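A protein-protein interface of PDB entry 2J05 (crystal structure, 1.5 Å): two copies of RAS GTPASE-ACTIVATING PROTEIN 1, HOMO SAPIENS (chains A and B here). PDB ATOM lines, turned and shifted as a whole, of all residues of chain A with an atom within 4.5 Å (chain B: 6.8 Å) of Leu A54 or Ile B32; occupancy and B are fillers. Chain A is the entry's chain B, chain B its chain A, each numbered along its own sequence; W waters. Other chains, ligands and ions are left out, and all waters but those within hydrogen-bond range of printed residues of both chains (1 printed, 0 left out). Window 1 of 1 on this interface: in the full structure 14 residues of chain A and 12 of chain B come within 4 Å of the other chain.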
ATOM      1  N   ASP A  21      -9.696  10.430   1.681  1.00  0.00           N
ATOM      2  CA  ASP A  21     -11.116  10.206   1.857  1.00  0.00           C
ATOM      3  C   ASP A  21     -11.509  10.087   3.317  1.00  0.00           C
ATOM      4  O   ASP A  21     -12.556   9.536   3.674  1.00  0.00           O
ATOM      5  CB  ASP A  21     -11.561   9.009   1.021  1.00  0.00           C
ATOM      6  CG  ASP A  21     -11.460   9.296  -0.474  1.00  0.00           C
ATOM      7  OD1 ASP A  21     -11.608  10.482  -0.869  1.00  0.00           O
ATOM      8  OD2 ASP A  21     -11.245   8.351  -1.258  1.00  0.00           O
ATOM      9  N   GLU A  22     -10.646  10.633   4.165  1.00  0.00           N
ATOM     10  CA  GLU A  22     -10.915  10.685   5.592  1.00  0.00           C
ATOM     11  C   GLU A  22     -11.905  11.821   5.827  1.00  0.00           C
ATOM     12  O   GLU A  22     -12.031  12.733   5.000  1.00  0.00           O
ATOM     13  CB  GLU A  22      -9.639  11.002   6.369  1.00  0.00           C
ATOM     14  CG  GLU A  22      -8.709   9.824   6.512  1.00  0.00           C
ATOM     15  CD  GLU A  22      -7.520  10.142   7.381  1.00  0.00           C
ATOM     16  OE1 GLU A  22      -7.378  11.313   7.802  1.00  0.00           O
ATOM     17  OE2 GLU A  22      -6.730   9.217   7.652  1.00  0.00           O
ATOM     18  N   ILE A  23     -12.607  11.758   6.953  1.00  0.00           N
ATOM     19  CA  ILE A  23     -13.547  12.808   7.314  1.00  0.00           C
ATOM     20  C   ILE A  23     -13.176  13.318   8.704  1.00  0.00           C
ATOM     21  O   ILE A  23     -12.628  12.587   9.526  1.00  0.00           O
ATOM     22  CB  ILE A  23     -15.007  12.314   7.304  1.00  0.00           C
ATOM     23  CG1 ILE A  23     -15.166  11.069   8.188  1.00  0.00           C
ATOM     24  CG2 ILE A  23     -15.438  12.032   5.861  1.00  0.00           C
ATOM     25  CD1 ILE A  23     -16.621  10.621   8.350  1.00  0.00           C
ATOM     26  N   LEU A  37     -12.866  -2.820   8.045  1.00  0.00           N
ATOM     27  CA  LEU A  37     -11.568  -2.621   7.374  1.00  0.00           C
ATOM     28  C   LEU A  37     -10.457  -3.290   8.186  1.00  0.00           C
ATOM     29  O   LEU A  37     -10.714  -4.183   8.985  1.00  0.00           O
ATOM     30  CB  LEU A  37     -11.238  -1.125   7.216  1.00  0.00           C
ATOM     31  CG  LEU A  37     -12.308  -0.227   6.586  1.00  0.00           C
ATOM     32  CD1 LEU A  37     -11.757   1.185   6.427  1.00  0.00           C
ATOM     33  CD2 LEU A  37     -12.728  -0.786   5.225  1.00  0.00           C
ATOM     34  N   TRP A  41      -8.624   1.361  11.173  1.00  0.00           N
ATOM     35  CA  TRP A  41      -9.445   2.190  10.293  1.00  0.00           C
ATOM     36  C   TRP A  41     -10.874   1.690  10.278  1.00  0.00           C
ATOM     37  O   TRP A  41     -11.132   0.562  10.638  1.00  0.00           O
ATOM     38  CB  TRP A  41      -8.943   2.102   8.849  1.00  0.00           C
ATOM     39  CG  TRP A  41      -7.498   2.327   8.665  1.00  0.00           C
ATOM     40  CD1 TRP A  41      -6.512   1.384   8.643  1.00  0.00           C
ATOM     41  CD2 TRP A  41      -6.861   3.584   8.439  1.00  0.00           C
ATOM     42  NE1 TRP A  41      -5.295   1.977   8.407  1.00  0.00           N
ATOM     43  CE2 TRP A  41      -5.480   3.329   8.278  1.00  0.00           C
ATOM     44  CE3 TRP A  41      -7.323   4.906   8.351  1.00  0.00           C
ATOM     45  CZ2 TRP A  41      -4.551   4.350   8.035  1.00  0.00           C
ATOM     46  CZ3 TRP A  41      -6.401   5.922   8.108  1.00  0.00           C
ATOM     47  CH2 TRP A  41      -5.031   5.636   7.953  1.00  0.00           C
ATOM     48  N   MET A  42     -11.796   2.542   9.836  1.00  0.00           N
ATOM     49  CA  MET A  42     -13.195   2.146   9.689  1.00  0.00           C
ATOM     50  C   MET A  42     -13.810   2.986   8.578  1.00  0.00           C
ATOM     51  O   MET A  42     -13.427   4.136   8.392  1.00  0.00           O
ATOM     52  CB  MET A  42     -14.014   2.387  10.966  1.00  0.00           C
ATOM     53  CG  MET A  42     -13.617   1.562  12.161  1.00  0.00           C
ATOM     54  SD  MET A  42     -14.782   2.020  13.652  1.00  0.00           S
ATOM     55  CE  MET A  42     -15.270   0.251  14.162  1.00  0.00           C
ATOM     56  N   TRP A  43     -14.764   2.411   7.846  1.00  0.00           N
ATOM     57  CA  TRP A  43     -15.476   3.133   6.779  1.00  0.00           C
ATOM     58  C   TRP A  43     -16.843   3.357   7.407  1.00  0.00           C
ATOM     59  O   TRP A  43     -17.551   2.405   7.745  1.00  0.00           O
ATOM     60  CB  TRP A  43     -15.579   2.278   5.516  1.00  0.00           C
ATOM     61  CG  TRP A  43     -16.203   2.986   4.334  1.00  0.00           C
ATOM     62  CD1 TRP A  43     -17.396   2.682   3.742  1.00  0.00           C
ATOM     63  CD2 TRP A  43     -15.649   4.076   3.585  1.00  0.00           C
ATOM     64  NE1 TRP A  43     -17.617   3.511   2.667  1.00  0.00           N
ATOM     65  CE2 TRP A  43     -16.562   4.377   2.546  1.00  0.00           C
ATOM     66  CE3 TRP A  43     -14.468   4.824   3.683  1.00  0.00           C
ATOM     67  CZ2 TRP A  43     -16.332   5.398   1.611  1.00  0.00           C
ATOM     68  CZ3 TRP A  43     -14.233   5.834   2.758  1.00  0.00           C
ATOM     69  CH2 TRP A  43     -15.166   6.114   1.728  1.00  0.00           C
ATOM     70  N   GLY A  53     -17.150   8.345   5.046  1.00  0.00           N
ATOM     71  CA  GLY A  53     -15.718   8.453   4.886  1.00  0.00           C
ATOM     72  C   GLY A  53     -14.911   7.549   5.789  1.00  0.00           C
ATOM     73  O   GLY A  53     -15.435   6.724   6.530  1.00  0.00           O
ATOM     74  N   LEU A  54     -13.603   7.749   5.731  1.00  0.00           N
ATOM     75  CA  LEU A  54     -12.658   6.958   6.484  1.00  0.00           C
ATOM     76  C   LEU A  54     -12.297   7.628   7.802  1.00  0.00           C
ATOM     77  O   LEU A  54     -12.061   8.841   7.839  1.00  0.00           O
ATOM     78  CB  LEU A  54     -11.406   6.779   5.619  1.00  0.00           C
ATOM     79  CG  LEU A  54     -10.213   5.976   6.113  1.00  0.00           C
ATOM     80  CD1 LEU A  54     -10.599   4.518   6.316  1.00  0.00           C
ATOM     81  CD2 LEU A  54      -9.098   6.106   5.073  1.00  0.00           C
ATOM     82  N   ILE A  55     -12.277   6.852   8.884  1.00  0.00           N
ATOM     83  CA  ILE A  55     -11.881   7.398  10.180  1.00  0.00           C
ATOM     84  C   ILE A  55     -10.869   6.481  10.859  1.00  0.00           C
ATOM     85  O   ILE A  55     -10.732   5.308  10.494  1.00  0.00           O
ATOM     86  CB  ILE A  55     -13.070   7.581  11.163  1.00  0.00           C
ATOM     87  CG1 ILE A  55     -13.721   6.228  11.476  1.00  0.00           C
ATOM     88  CG2 ILE A  55     -14.057   8.607  10.611  1.00  0.00           C
ATOM     89  CD1 ILE A  55     -14.707   6.301  12.630  1.00  0.00           C
ATOM     90  N   HIS B   3      -2.438   6.825  -3.405  1.00  0.00           N
ATOM     91  CA  HIS B   3      -3.816   6.398  -3.206  1.00  0.00           C
ATOM     92  C   HIS B   3      -4.040   6.106  -1.724  1.00  0.00           C
ATOM     93  O   HIS B   3      -5.084   5.607  -1.330  1.00  0.00           O
ATOM     94  CB  HIS B   3      -4.105   5.139  -4.031  1.00  0.00           C
ATOM     95  CG  HIS B   3      -3.922   5.330  -5.504  1.00  0.00           C
ATOM     96  ND1 HIS B   3      -4.498   6.375  -6.195  1.00  0.00           N
ATOM     97  CD2 HIS B   3      -3.237   4.605  -6.421  1.00  0.00           C
ATOM     98  CE1 HIS B   3      -4.177   6.285  -7.474  1.00  0.00           C
ATOM     99  NE2 HIS B   3      -3.414   5.220  -7.638  1.00  0.00           N
ATOM    100  N   MET B   4      -3.042   6.422  -0.907  1.00  0.00           N
ATOM    101  CA  MET B   4      -3.129   6.189   0.525  1.00  0.00           C
ATOM    102  C   MET B   4      -4.369   6.847   1.122  1.00  0.00           C
ATOM    103  O   MET B   4      -4.654   7.999   0.825  1.00  0.00           O
ATOM    104  CB  MET B   4      -1.876   6.745   1.209  1.00  0.00           C
ATOM    105  CG  MET B   4      -1.875   6.547   2.697  1.00  0.00           C
ATOM    106  SD  MET B   4      -1.852   4.670   3.078  1.00  0.00           S
ATOM    107  CE  MET B   4      -0.301   4.637   4.242  1.00  0.00           C
ATOM    108  N   ARG B   5      -5.095   6.108   1.958  1.00  0.00           N
ATOM    109  CA  ARG B   5      -6.298   6.632   2.618  1.00  0.00           C
ATOM    110  C   ARG B   5      -7.401   7.045   1.644  1.00  0.00           C
ATOM    111  O   ARG B   5      -8.211   7.919   1.956  1.00  0.00           O
ATOM    112  CB  ARG B   5      -5.953   7.852   3.475  1.00  0.00           C
ATOM    113  CG  ARG B   5      -5.008   7.615   4.635  1.00  0.00           C
ATOM    114  CD  ARG B   5      -4.836   8.927   5.392  1.00  0.00           C
ATOM    115  NE  ARG B   5      -4.184   8.770   6.689  1.00  0.00           N
ATOM    116  CZ  ARG B   5      -2.887   8.535   6.854  1.00  0.00           C
ATOM    117  NH1 ARG B   5      -2.088   8.426   5.797  1.00  0.00           N
ATOM    118  NH2 ARG B   5      -2.389   8.412   8.078  1.00  0.00           N
ATOM    119  N   ARG B   6      -7.435   6.426   0.473  1.00  0.00           N
ATOM    120  CA  ARG B   6      -8.452   6.754  -0.529  1.00  0.00           C
ATOM    121  C   ARG B   6      -9.273   5.537  -0.902  1.00  0.00           C
ATOM    122  O   ARG B   6      -8.831   4.396  -0.724  1.00  0.00           O
ATOM    123  CB  ARG B   6      -7.802   7.302  -1.810  1.00  0.00           C
ATOM    124  CG  ARG B   6      -7.093   8.649  -1.664  1.00  0.00           C
ATOM    125  CD  ARG B   6      -8.078   9.756  -1.350  1.00  0.00           C
ATOM    126  NE  ARG B   6      -8.950  10.080  -2.478  1.00  0.00           N
ATOM    127  CZ  ARG B   6      -8.594  10.837  -3.514  1.00  0.00           C
ATOM    128  NH1 ARG B   6      -7.375  11.360  -3.571  1.00  0.00           N
ATOM    129  NH2 ARG B   6      -9.458  11.071  -4.495  1.00  0.00           N
ATOM    130  N   ARG B   7     -10.482   5.786  -1.396  1.00  0.00           N
ATOM    131  CA  ARG B   7     -11.340   4.708  -1.881  1.00  0.00           C
ATOM    132  C   ARG B   7     -11.061   4.631  -3.381  1.00  0.00           C
ATOM    133  O   ARG B   7     -11.075   5.649  -4.090  1.00  0.00           O
ATOM    134  CB  ARG B   7     -12.827   5.004  -1.647  1.00  0.00           C
ATOM    135  CG  ARG B   7     -13.746   3.883  -2.164  1.00  0.00           C
ATOM    136  CD  ARG B   7     -15.189   4.055  -1.710  1.00  0.00           C
ATOM    137  NE  ARG B   7     -15.805   5.244  -2.280  1.00  0.00           N
ATOM    138  CZ  ARG B   7     -17.118   5.449  -2.323  1.00  0.00           C
ATOM    139  NH1 ARG B   7     -17.951   4.540  -1.827  1.00  0.00           N
ATOM    140  NH2 ARG B   7     -17.601   6.557  -2.869  1.00  0.00           N
ATOM    141  N   VAL B   8     -10.776   3.422  -3.850  1.00  0.00           N
ATOM    142  CA  VAL B   8     -10.476   3.187  -5.255  1.00  0.00           C
ATOM    143  C   VAL B   8     -11.429   2.123  -5.807  1.00  0.00           C
ATOM    144  O   VAL B   8     -12.000   1.338  -5.057  1.00  0.00           O
ATOM    145  CB  VAL B   8      -8.998   2.754  -5.431  1.00  0.00           C
ATOM    146  CG1 VAL B   8      -8.068   3.871  -4.974  1.00  0.00           C
ATOM    147  CG2 VAL B   8      -8.721   1.495  -4.630  1.00  0.00           C
ATOM    148  N   MET B  30     -15.001  -1.907  -4.817  1.00  0.00           N
ATOM    149  CA  MET B  30     -14.327  -0.751  -4.264  1.00  0.00           C
ATOM    150  C   MET B  30     -13.463  -1.175  -3.090  1.00  0.00           C
ATOM    151  O   MET B  30     -13.742  -2.180  -2.450  1.00  0.00           O
ATOM    152  CB  MET B  30     -15.345   0.312  -3.887  1.00  0.00           C
ATOM    153  CG  MET B  30     -16.031   0.808  -5.139  1.00  0.00           C
ATOM    154  SD  MET B  30     -16.885   2.484  -4.923  1.00  0.00           S
ATOM    155  CE  MET B  30     -18.459   1.836  -4.017  1.00  0.00           C
ATOM    156  N   PHE B  31     -12.402  -0.418  -2.841  1.00  0.00           N
ATOM    157  CA  PHE B  31     -11.437  -0.758  -1.793  1.00  0.00           C
ATOM    158  C   PHE B  31     -10.945   0.488  -1.077  1.00  0.00           C
ATOM    159  O   PHE B  31     -10.990   1.586  -1.626  1.00  0.00           O
ATOM    160  CB  PHE B  31     -10.169  -1.395  -2.398  1.00  0.00           C
ATOM    161  CG  PHE B  31     -10.418  -2.452  -3.431  1.00  0.00           C
ATOM    162  CD1 PHE B  31     -10.329  -3.799  -3.097  1.00  0.00           C
ATOM    163  CD2 PHE B  31     -10.706  -2.104  -4.747  1.00  0.00           C
ATOM    164  CE1 PHE B  31     -10.523  -4.798  -4.058  1.00  0.00           C
ATOM    165  CE2 PHE B  31     -10.901  -3.091  -5.714  1.00  0.00           C
ATOM    166  CZ  PHE B  31     -10.810  -4.443  -5.365  1.00  0.00           C
ATOM    167  N   ILE B  32     -10.462   0.301   0.147  1.00  0.00           N
ATOM    168  CA  ILE B  32      -9.854   1.390   0.898  1.00  0.00           C
ATOM    169  C   ILE B  32      -8.377   1.005   0.972  1.00  0.00           C
ATOM    170  O   ILE B  32      -8.041  -0.111   1.356  1.00  0.00           O
ATOM    171  CB  ILE B  32     -10.424   1.520   2.325  1.00  0.00           C
ATOM    172  CG1 ILE B  32     -11.909   1.898   2.277  1.00  0.00           C
ATOM    173  CG2 ILE B  32      -9.613   2.547   3.104  1.00  0.00           C
ATOM    174  CD1 ILE B  32     -12.200   3.145   1.470  1.00  0.00           C
ATOM    175  N   VAL B  33      -7.501   1.920   0.581  1.00  0.00           N
ATOM    176  CA  VAL B  33      -6.068   1.671   0.588  1.00  0.00           C
ATOM    177  C   VAL B  33      -5.442   1.932   1.961  1.00  0.00           C
ATOM    178  O   VAL B  33      -5.524   3.042   2.482  1.00  0.00           O
ATOM    179  CB  VAL B  33      -5.371   2.544  -0.473  1.00  0.00           C
ATOM    180  CG1 VAL B  33      -3.867   2.284  -0.458  1.00  0.00           C
ATOM    181  CG2 VAL B  33      -5.946   2.229  -1.859  1.00  0.00           C
ATOM    182  N   HIS B  34      -4.812   0.907   2.537  1.00  0.00           N
ATOM    183  CA  HIS B  34      -4.187   1.039   3.858  1.00  0.00           C
ATOM    184  C   HIS B  34      -2.676   1.255   3.814  1.00  0.00           C
ATOM    185  O   HIS B  34      -2.126   1.973   4.649  1.00  0.00           O
ATOM    186  CB  HIS B  34      -4.488  -0.205   4.702  1.00  0.00           C
ATOM    187  CG  HIS B  34      -5.945  -0.520   4.814  1.00  0.00           C
ATOM    188  ND1 HIS B  34      -6.883   0.421   5.186  1.00  0.00           N
ATOM    189  CD2 HIS B  34      -6.623  -1.673   4.610  1.00  0.00           C
ATOM    190  CE1 HIS B  34      -8.079  -0.141   5.205  1.00  0.00           C
ATOM    191  NE2 HIS B  34      -7.948  -1.413   4.861  1.00  0.00           N
ATOM    192  N   ASN B  35      -2.012   0.607   2.862  1.00  0.00           N
ATOM    193  CA  ASN B  35      -0.569   0.717   2.700  1.00  0.00           C
ATOM    194  C   ASN B  35      -0.231   0.708   1.217  1.00  0.00           C
ATOM    195  O   ASN B  35      -0.809  -0.061   0.443  1.00  0.00           O
ATOM    196  CB  ASN B  35       0.172  -0.477   3.317  1.00  0.00           C
ATOM    197  CG  ASN B  35      -0.179  -0.718   4.765  1.00  0.00           C
ATOM    198  OD1 ASN B  35      -1.250  -1.232   5.089  1.00  0.00           O
ATOM    199  ND2 ASN B  35       0.744  -0.367   5.648  1.00  0.00           N
ATOM    200  N   TRP B  43      -1.901  -2.733   0.176  1.00  0.00           N
ATOM    201  CA  TRP B  43      -2.655  -3.552   1.117  1.00  0.00           C
ATOM    202  C   TRP B  43      -3.963  -2.783   1.271  1.00  0.00           C
ATOM    203  O   TRP B  43      -3.960  -1.588   1.582  1.00  0.00           O
ATOM    204  CB  TRP B  43      -1.933  -3.651   2.463  1.00  0.00           C
ATOM    205  CG  TRP B  43      -2.620  -4.578   3.431  1.00  0.00           C
ATOM    206  CD1 TRP B  43      -3.307  -4.225   4.564  1.00  0.00           C
ATOM    207  CD2 TRP B  43      -2.685  -6.006   3.352  1.00  0.00           C
ATOM    208  NE1 TRP B  43      -3.794  -5.348   5.194  1.00  0.00           N
ATOM    209  CE2 TRP B  43      -3.428  -6.455   4.473  1.00  0.00           C
ATOM    210  CE3 TRP B  43      -2.188  -6.954   2.447  1.00  0.00           C
ATOM    211  CZ2 TRP B  43      -3.685  -7.811   4.710  1.00  0.00           C
ATOM    212  CZ3 TRP B  43      -2.444  -8.304   2.684  1.00  0.00           C
ATOM    213  CH2 TRP B  43      -3.185  -8.717   3.805  1.00  0.00           C
ATOM    214  N   VAL B  44      -5.077  -3.475   1.052  1.00  0.00           N
ATOM    215  CA  VAL B  44      -6.386  -2.833   1.055  1.00  0.00           C
ATOM    216  C   VAL B  44      -7.480  -3.698   1.657  1.00  0.00           C
ATOM    217  O   VAL B  44      -7.267  -4.860   1.998  1.00  0.00           O
ATOM    218  CB  VAL B  44      -6.850  -2.565  -0.413  1.00  0.00           C
ATOM    219  CG1 VAL B  44      -5.760  -1.816  -1.204  1.00  0.00           C
ATOM    220  CG2 VAL B  44      -7.195  -3.894  -1.109  1.00  0.00           C
ATOM    221  N   THR B  45      -8.666  -3.105   1.772  1.00  0.00           N
ATOM    222  CA  THR B  45      -9.846  -3.846   2.185  1.00  0.00           C
ATOM    223  C   THR B  45     -10.831  -3.719   1.025  1.00  0.00           C
ATOM    224  O   THR B  45     -11.051  -2.610   0.515  1.00  0.00           O
ATOM    225  CB  THR B  45     -10.566  -3.264   3.418  1.00  0.00           C
ATOM    226  OG1 THR B  45      -9.739  -3.406   4.575  1.00  0.00           O
ATOM    227  CG2 THR B  45     -11.897  -4.020   3.661  1.00  0.00           C
ATOM    228  N   ASN B  46     -11.389  -4.847   0.589  1.00  0.00           N
ATOM    229  CA  ASN B  46     -12.410  -4.861  -0.461  1.00  0.00           C
ATOM    230  C   ASN B  46     -13.701  -4.589   0.320  1.00  0.00           C
ATOM    231  O   ASN B  46     -14.071  -5.360   1.205  1.00  0.00           O
ATOM    232  CB  ASN B  46     -12.481  -6.237  -1.118  1.00  0.00           C
ATOM    233  CG  ASN B  46     -13.513  -6.300  -2.233  1.00  0.00           C
ATOM    234  OD1 ASN B  46     -14.611  -5.767  -2.108  1.00  0.00           O
ATOM    235  ND2 ASN B  46     -13.167  -6.971  -3.317  1.00  0.00           N
ATOM    236  N   LEU B  47     -14.361  -3.480   0.001  1.00  0.00           N
ATOM    237  CA  LEU B  47     -15.569  -3.073   0.709  1.00  0.00           C
ATOM    238  C   LEU B  47     -16.777  -3.982   0.527  1.00  0.00           C
ATOM    239  O   LEU B  47     -17.702  -3.967   1.340  1.00  0.00           O
ATOM    240  CB  LEU B  47     -15.929  -1.642   0.322  1.00  0.00           C
ATOM    241  CG  LEU B  47     -14.946  -0.559   0.779  1.00  0.00           C
ATOM    242  CD1 LEU B  47     -15.326   0.778   0.172  1.00  0.00           C
ATOM    243  CD2 LEU B  47     -14.956  -0.465   2.301  1.00  0.00           C
ATOM    244  N   ARG B  65     -15.109   9.879  -1.925  1.00  0.00           N
ATOM    245  CA  ARG B  65     -16.055   9.466  -0.890  1.00  0.00           C
ATOM    246  C   ARG B  65     -17.481   9.202  -1.382  1.00  0.00           C
ATOM    247  O   ARG B  65     -18.212   8.470  -0.672  1.00  0.00           O
ATOM    248  CB  ARG B  65     -16.102  10.520   0.225  1.00  0.00           C
ATOM    249  CG  ARG B  65     -14.788  10.718   0.957  1.00  0.00           C
ATOM    250  CD  ARG B  65     -14.967  11.552   2.234  1.00  0.00           C
ATOM    251  NE  ARG B  65     -15.415  12.921   1.978  1.00  0.00           N
ATOM    252  CZ  ARG B  65     -16.673  13.344   2.094  1.00  0.00           C
ATOM    253  NH1 ARG B  65     -17.641  12.513   2.467  1.00  0.00           N
ATOM    254  NH2 ARG B  65     -16.969  14.613   1.828  1.00  0.00           N
ATOM    255  OXT ARG B  65     -17.861   9.742  -2.445  1.00  0.00           O
HETATM  256  O   HOH W   1     -10.558   8.363  -3.854  1.00  0.00           O
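The backbone carbonyl oxygen (O) of Arg B5 is in hydrogen-bond range of the backbone NH (N) of Asp A21, at 2.9 Å.
NE of Arg B5 is in salt-bridge range of OE2 of Glu A22 (2.8 Å).
OD2 of Asp A21 is in salt-bridge range of NE of Arg B6 (3.1 Å).
N of Arg B7 lies within hydrogen-bond range of OD2 of Asp A21 (2.7 Å).
The guanidinium group (NH2) of Arg B7 is in salt-bridge range of the chain-end carboxylate (O) of Arg B65 (3.0 Å).
The backbone NH (N) of Leu B47 lies within hydrogen-bond range of the backbone carbonyl oxygen (O) of Met B30.
N of Ile B32 sits at hydrogen-bond distance from O of Thr B45, at 3.0 Å.
The backbone NH (N) of His B34 sits at hydrogen-bond distance from the backbone carbonyl oxygen (O) of Trp B43.
OG1 of Thr B45 sits at hydrogen-bond distance from NE2 of His B34 (2.7 Å).
The backbone NH (N) of Leu A54 lies within hydrogen-bond range of the backbone carbonyl oxygen (O) of Asp A21, at 2.9 Å.
CG2 of Ile A23 touches CD of Arg B65, at 3.7 Å.
Leu A37 touches His B34.
Thr B45 touches Leu A37 (OG1 to CA, 3.4 Å).
CD2 of Leu A37 touches CD2 of Leu B47, 3.7 Å away.
NE of Arg B5 touches CH2 of Trp A41, 3.5 Å away.
His B34 touches Trp A41.
CZ2 of Trp A43 touches CD of Arg B7, 3.8 Å away.
Trp A43 touches Ile B32.
CD2 of Leu A54 touches O of Arg B5, at 3.7 Å.
CG2 of Ile B32 touches CD1 of Leu A54 (3.9 Å).
Of the printed residues of chain B, Glu A22 touches Arg B5 (2.8 Å).
Of the printed residues of chain B, Trp A43 touches Arg B7 (3.8 Å) and Ile B32 (3.6 Å).
Leu A54 touches just these residues of chain B: Arg B5 (3.7 Å) and Ile B32 (3.9 Å).
Met B30 touches none of the printed residues of chain A.
Of chain A, only Trp A43 and Leu A54 come within 4 Å of Ile B32.
Of the printed residues of chain A, His B34 touches Leu A37 and Trp A41.
Val B44 touches none of the printed residues of chain A.
The nearest residue of chain A that does not touch Ile B32 is Leu A37 (4.1 Å).
The nearest printed residue of chain A that does not touch Arg B65 is Gly A53 (4.1 Å).
Hydrophobic or aromatic side chains of chain A within 4 Å of the printed part of chain B: Ile A23, Leu A37, Trp A41, Trp A43 and Leu A54.
Among the printed residues, Asp or Glu carboxylates within 4 Å of a Lys or Arg side-chain nitrogen of the other chain: Asp A21 with Arg B6 and Glu A22 with Arg B5.
1 position is printed for both chains.
Of the 15 pairs that touch across the chains among the printed residues, none has its exchanged pair printed and touching as well.
Water W1 lies within hydrogen-bond range of OD2 of Asp A21, NE of Arg B6 and O of Arg B7.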
